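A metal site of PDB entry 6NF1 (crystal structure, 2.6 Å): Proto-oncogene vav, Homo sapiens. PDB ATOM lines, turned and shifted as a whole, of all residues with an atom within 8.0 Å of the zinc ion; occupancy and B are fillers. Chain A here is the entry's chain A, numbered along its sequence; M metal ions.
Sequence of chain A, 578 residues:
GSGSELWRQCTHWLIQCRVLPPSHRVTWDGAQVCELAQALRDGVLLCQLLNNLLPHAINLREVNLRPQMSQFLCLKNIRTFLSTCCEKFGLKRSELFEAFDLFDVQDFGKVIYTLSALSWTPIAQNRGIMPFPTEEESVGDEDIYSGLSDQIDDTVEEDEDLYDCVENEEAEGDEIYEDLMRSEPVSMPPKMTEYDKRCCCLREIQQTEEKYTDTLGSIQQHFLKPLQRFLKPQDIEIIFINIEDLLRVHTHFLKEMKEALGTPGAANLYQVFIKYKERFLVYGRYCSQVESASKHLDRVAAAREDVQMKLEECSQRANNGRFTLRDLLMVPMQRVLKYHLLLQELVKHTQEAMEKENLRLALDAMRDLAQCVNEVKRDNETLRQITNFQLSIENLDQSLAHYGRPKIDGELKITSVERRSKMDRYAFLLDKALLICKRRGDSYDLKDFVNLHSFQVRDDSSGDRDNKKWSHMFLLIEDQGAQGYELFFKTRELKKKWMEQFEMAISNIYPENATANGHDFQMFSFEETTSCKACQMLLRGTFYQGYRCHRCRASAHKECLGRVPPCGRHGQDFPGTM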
ATOM      1  N   SER A 531      14.301   4.116  11.493  1.00  0.00           N
ATOM      2  CA  SER A 531      14.471   4.050  10.046  1.00  0.00           C
ATOM      3  C   SER A 531      13.421   4.921   9.391  1.00  0.00           C
ATOM      4  O   SER A 531      12.319   5.074   9.914  1.00  0.00           O
ATOM      5  CB  SER A 531      14.338   2.608   9.553  1.00  0.00           C
ATOM      6  OG  SER A 531      15.394   1.792  10.019  1.00  0.00           O
ATOM      7  N   CYS A 532      13.771   5.506   8.240  1.00  0.00           N
ATOM      8  CA  CYS A 532      12.898   6.364   7.446  1.00  0.00           C
ATOM      9  C   CYS A 532      11.708   5.536   6.911  1.00  0.00           C
ATOM     10  O   CYS A 532      11.910   4.477   6.306  1.00  0.00           O
ATOM     11  CB  CYS A 532      13.685   7.022   6.317  1.00  0.00           C
ATOM     12  SG  CYS A 532      12.735   8.204   5.337  1.00  0.00           S
ATOM     13  N   LYS A 533      10.468   5.995   7.170  1.00  0.00           N
ATOM     14  CA  LYS A 533       9.248   5.308   6.708  1.00  0.00           C
ATOM     15  C   LYS A 533       9.095   5.335   5.163  1.00  0.00           C
ATOM     16  O   LYS A 533       8.327   4.542   4.615  1.00  0.00           O
ATOM     17  CB  LYS A 533       7.970   5.859   7.406  1.00  0.00           C
ATOM     18  CG  LYS A 533       8.050   5.918   8.933  1.00  0.00           C
ATOM     19  CD  LYS A 533       7.830   4.554   9.588  1.00  0.00           C
ATOM     20  CE  LYS A 533       7.871   4.603  11.091  1.00  0.00           C
ATOM     21  NZ  LYS A 533       9.259   4.666  11.616  1.00  0.00           N
ATOM     22  N   ALA A 534       9.869   6.217   4.477  1.00  0.00           N
ATOM     23  CA  ALA A 534       9.884   6.401   3.036  1.00  0.00           C
ATOM     24  C   ALA A 534      10.980   5.628   2.289  1.00  0.00           C
ATOM     25  O   ALA A 534      10.675   4.870   1.359  1.00  0.00           O
ATOM     26  CB  ALA A 534       9.954   7.887   2.698  1.00  0.00           C
ATOM     27  N   CYS A 535      12.263   5.833   2.653  1.00  0.00           N
ATOM     28  CA  CYS A 535      13.383   5.194   1.948  1.00  0.00           C
ATOM     29  C   CYS A 535      13.956   3.935   2.653  1.00  0.00           C
ATOM     30  O   CYS A 535      14.872   3.307   2.107  1.00  0.00           O
ATOM     31  CB  CYS A 535      14.488   6.212   1.641  1.00  0.00           C
ATOM     32  SG  CYS A 535      15.492   6.684   3.072  1.00  0.00           S
ATOM     33  N   GLN A 536      13.390   3.549   3.835  1.00  0.00           N
ATOM     34  CA  GLN A 536      13.774   2.370   4.650  1.00  0.00           C
ATOM     35  C   GLN A 536      15.195   2.449   5.274  1.00  0.00           C
ATOM     36  O   GLN A 536      15.571   1.565   6.047  1.00  0.00           O
ATOM     37  CB  GLN A 536      13.598   1.032   3.871  1.00  0.00           C
ATOM     38  CG  GLN A 536      12.295   0.867   3.075  1.00  0.00           C
ATOM     39  CD  GLN A 536      11.172   0.320   3.913  1.00  0.00           C
ATOM     40  OE1 GLN A 536      10.693   0.961   4.868  1.00  0.00           O
ATOM     41  NE2 GLN A 536      10.698  -0.871   3.561  1.00  0.00           N
ATOM     42  N   MET A 537      15.963   3.502   4.932  1.00  0.00           N
ATOM     43  CA  MET A 537      17.337   3.725   5.396  1.00  0.00           C
ATOM     44  C   MET A 537      17.401   4.333   6.803  1.00  0.00           C
ATOM     45  O   MET A 537      16.493   5.017   7.238  1.00  0.00           O
ATOM     46  CB  MET A 537      18.102   4.609   4.411  1.00  0.00           C
ATOM     47  CG  MET A 537      18.262   3.992   3.050  1.00  0.00           C
ATOM     48  SD  MET A 537      19.190   2.453   3.087  1.00  0.00           S
ATOM     49  CE  MET A 537      20.857   3.082   3.155  1.00  0.00           C
ATOM     50  N   LEU A 538      18.511   4.089   7.511  1.00  0.00           N
ATOM     51  CA  LEU A 538      18.732   4.571   8.875  1.00  0.00           C
ATOM     52  C   LEU A 538      18.721   6.088   8.956  1.00  0.00           C
ATOM     53  O   LEU A 538      19.236   6.767   8.077  1.00  0.00           O
ATOM     54  CB  LEU A 538      20.068   4.002   9.431  1.00  0.00           C
ATOM     55  CG  LEU A 538      20.426   4.285  10.908  1.00  0.00           C
ATOM     56  CD1 LEU A 538      19.709   3.358  11.841  1.00  0.00           C
ATOM     57  CD2 LEU A 538      21.936   4.202  11.154  1.00  0.00           C
ATOM     58  N   LEU A 539      18.123   6.620  10.033  1.00  0.00           N
ATOM     59  CA  LEU A 539      18.155   8.049  10.321  1.00  0.00           C
ATOM     60  C   LEU A 539      19.463   8.206  11.096  1.00  0.00           C
ATOM     61  O   LEU A 539      19.500   8.071  12.307  1.00  0.00           O
ATOM     62  CB  LEU A 539      16.913   8.445  11.153  1.00  0.00           C
ATOM     63  CG  LEU A 539      15.901   9.348  10.425  1.00  0.00           C
ATOM     64  CD1 LEU A 539      15.247   8.624   9.268  1.00  0.00           C
ATOM     65  CD2 LEU A 539      14.848   9.812  11.363  1.00  0.00           C
ATOM     66  N   ARG A 540      20.562   8.374  10.351  1.00  0.00           N
ATOM     67  CA  ARG A 540      21.946   8.380  10.819  1.00  0.00           C
ATOM     68  C   ARG A 540      22.319   9.526  11.799  1.00  0.00           C
ATOM     69  O   ARG A 540      21.987  10.690  11.559  1.00  0.00           O
ATOM     70  CB  ARG A 540      22.904   8.380   9.610  1.00  0.00           C
ATOM     71  CG  ARG A 540      22.715   7.203   8.636  1.00  0.00           C
ATOM     72  CD  ARG A 540      23.538   7.301   7.358  1.00  0.00           C
ATOM     73  NE  ARG A 540      22.748   7.738   6.203  1.00  0.00           N
ATOM     74  CZ  ARG A 540      22.000   6.940   5.448  1.00  0.00           C
ATOM     75  NH1 ARG A 540      21.911   5.643   5.726  1.00  0.00           N
ATOM     76  NH2 ARG A 540      21.309   7.431   4.439  1.00  0.00           N
ATOM     77  N   SER A 555       8.661   8.656  11.151  1.00  0.00           N
ATOM     78  CA  SER A 555       9.973   9.270  11.188  1.00  0.00           C
ATOM     79  C   SER A 555      10.576   9.272   9.792  1.00  0.00           C
ATOM     80  O   SER A 555      10.573   8.230   9.119  1.00  0.00           O
ATOM     81  CB  SER A 555      10.873   8.563  12.180  1.00  0.00           C
ATOM     82  OG  SER A 555      11.198   7.234  11.813  1.00  0.00           O
ATOM     83  N   ALA A 556      11.086  10.436   9.340  1.00  0.00           N
ATOM     84  CA  ALA A 556      11.669  10.544   8.017  1.00  0.00           C
ATOM     85  C   ALA A 556      12.875  11.460   7.945  1.00  0.00           C
ATOM     86  O   ALA A 556      13.125  12.223   8.881  1.00  0.00           O
ATOM     87  CB  ALA A 556      10.607  11.013   7.026  1.00  0.00           C
ATOM     88  N   HIS A 557      13.627  11.382   6.809  1.00  0.00           N
ATOM     89  CA  HIS A 557      14.729  12.269   6.453  1.00  0.00           C
ATOM     90  C   HIS A 557      14.069  13.532   5.865  1.00  0.00           C
ATOM     91  O   HIS A 557      12.967  13.421   5.314  1.00  0.00           O
ATOM     92  CB  HIS A 557      15.601  11.633   5.360  1.00  0.00           C
ATOM     93  CG  HIS A 557      16.354  10.409   5.784  1.00  0.00           C
ATOM     94  ND1 HIS A 557      16.149   9.190   5.172  1.00  0.00           N
ATOM     95  CD2 HIS A 557      17.325  10.273   6.714  1.00  0.00           C
ATOM     96  CE1 HIS A 557      16.967   8.345   5.770  1.00  0.00           C
ATOM     97  NE2 HIS A 557      17.695   8.948   6.700  1.00  0.00           N
ATOM     98  N   LYS A 558      14.712  14.721   5.981  1.00  0.00           N
ATOM     99  CA  LYS A 558      14.200  15.987   5.441  1.00  0.00           C
ATOM    100  C   LYS A 558      13.765  15.868   3.974  1.00  0.00           C
ATOM    101  O   LYS A 558      12.706  16.366   3.611  1.00  0.00           O
ATOM    102  CB  LYS A 558      15.266  17.109   5.564  1.00  0.00           C
ATOM    103  CG  LYS A 558      14.677  18.513   5.395  1.00  0.00           C
ATOM    104  CD  LYS A 558      15.717  19.597   5.371  1.00  0.00           C
ATOM    105  CE  LYS A 558      15.118  20.900   4.922  1.00  0.00           C
ATOM    106  NZ  LYS A 558      16.125  21.994   4.921  1.00  0.00           N
ATOM    107  N   GLU A 559      14.579  15.216   3.152  1.00  0.00           N
ATOM    108  CA  GLU A 559      14.355  15.030   1.716  1.00  0.00           C
ATOM    109  C   GLU A 559      13.375  13.916   1.389  1.00  0.00           C
ATOM    110  O   GLU A 559      13.124  13.676   0.210  1.00  0.00           O
ATOM    111  CB  GLU A 559      15.708  14.802   1.000  1.00  0.00           C
ATOM    112  CG  GLU A 559      16.328  13.408   1.182  1.00  0.00           C
ATOM    113  CD  GLU A 559      17.123  13.083   2.428  1.00  0.00           C
ATOM    114  OE1 GLU A 559      17.130  13.884   3.400  1.00  0.00           O
ATOM    115  OE2 GLU A 559      17.753  11.995   2.448  1.00  0.00           O
ATOM    116  N   CYS A 560      12.837  13.225   2.399  1.00  0.00           N
ATOM    117  CA  CYS A 560      11.952  12.077   2.187  1.00  0.00           C
ATOM    118  C   CYS A 560      10.475  12.317   2.537  1.00  0.00           C
ATOM    119  O   CYS A 560       9.653  11.434   2.294  1.00  0.00           O
ATOM    120  CB  CYS A 560      12.488  10.857   2.919  1.00  0.00           C
ATOM    121  SG  CYS A 560      14.096  10.287   2.320  1.00  0.00           S
ATOM    122  N   LEU A 561      10.151  13.492   3.107  1.00  0.00           N
ATOM    123  CA  LEU A 561       8.795  13.852   3.559  1.00  0.00           C
ATOM    124  C   LEU A 561       7.696  13.668   2.482  1.00  0.00           C
ATOM    125  O   LEU A 561       6.588  13.251   2.808  1.00  0.00           O
ATOM    126  CB  LEU A 561       8.778  15.261   4.145  1.00  0.00           C
ATOM    127  CG  LEU A 561       9.792  15.564   5.256  1.00  0.00           C
ATOM    128  CD1 LEU A 561       9.918  17.021   5.466  1.00  0.00           C
ATOM    129  CD2 LEU A 561       9.451  14.891   6.568  1.00  0.00           C
ATOM    130  N   ARG A 563       7.591  11.325   0.010  1.00  0.00           N
ATOM    131  CA  ARG A 563       7.425   9.878  -0.188  1.00  0.00           C
ATOM    132  C   ARG A 563       6.874   9.099   1.051  1.00  0.00           C
ATOM    133  O   ARG A 563       6.973   7.875   1.094  1.00  0.00           O
ATOM    134  CB  ARG A 563       8.765   9.274  -0.659  1.00  0.00           C
ATOM    135  CG  ARG A 563       9.406   9.984  -1.858  1.00  0.00           C
ATOM    136  CD  ARG A 563      10.340   9.077  -2.623  1.00  0.00           C
ATOM    137  NE  ARG A 563      10.637   9.601  -3.962  1.00  0.00           N
ATOM    138  CZ  ARG A 563      11.006   8.852  -4.992  1.00  0.00           C
ATOM    139  NH1 ARG A 563      11.126   7.533  -4.875  1.00  0.00           N
ATOM    140  NH2 ARG A 563      11.245   9.421  -6.174  1.00  0.00           N
ATOM    141  N   VAL A 564       6.252   9.800   2.022  1.00  0.00           N
ATOM    142  CA  VAL A 564       5.701   9.146   3.223  1.00  0.00           C
ATOM    143  C   VAL A 564       4.169   8.915   3.095  1.00  0.00           C
ATOM    144  O   VAL A 564       3.438   9.886   2.887  1.00  0.00           O
ATOM    145  CB  VAL A 564       6.082   9.908   4.527  1.00  0.00           C
ATOM    146  CG1 VAL A 564       5.518   9.219   5.774  1.00  0.00           C
ATOM    147  CG2 VAL A 564       7.582  10.091   4.663  1.00  0.00           C
HETATM  148 ZN    ZN M   1      14.417   8.637   4.012  1.00  0.00          ZN
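O of Met 537 sits at hydrogen-bond distance from N of Cys 532 (2.9 Å). The backbone NH of Met 537 sits close to the side-chain sulfur of Cys 535, 3.7 Å away. O of Leu 538 sits at hydrogen-bond distance from NE2 of His 557, at 3.0 Å. The side-chain sulfur (SG) of Cys 532 lies close to the backbone NH (N) of Ala 534 (3.6 Å).
Of the 19 residues printed, 4 come within 4 Å of the zinc ion. Along chain A the residues within 4 Å of the zinc ion span positions 532 to 560.
ND1 of His 557 is bound to the zinc ion, 2.2 Å away. SG of Cys 532 binds the zinc ion (2.2 Å). SG of Cys 560 binds the zinc ion. SG of Cys 535 is bound to the zinc ion, 2.4 Å away. The zinc ion has four donor atoms within binding distance.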
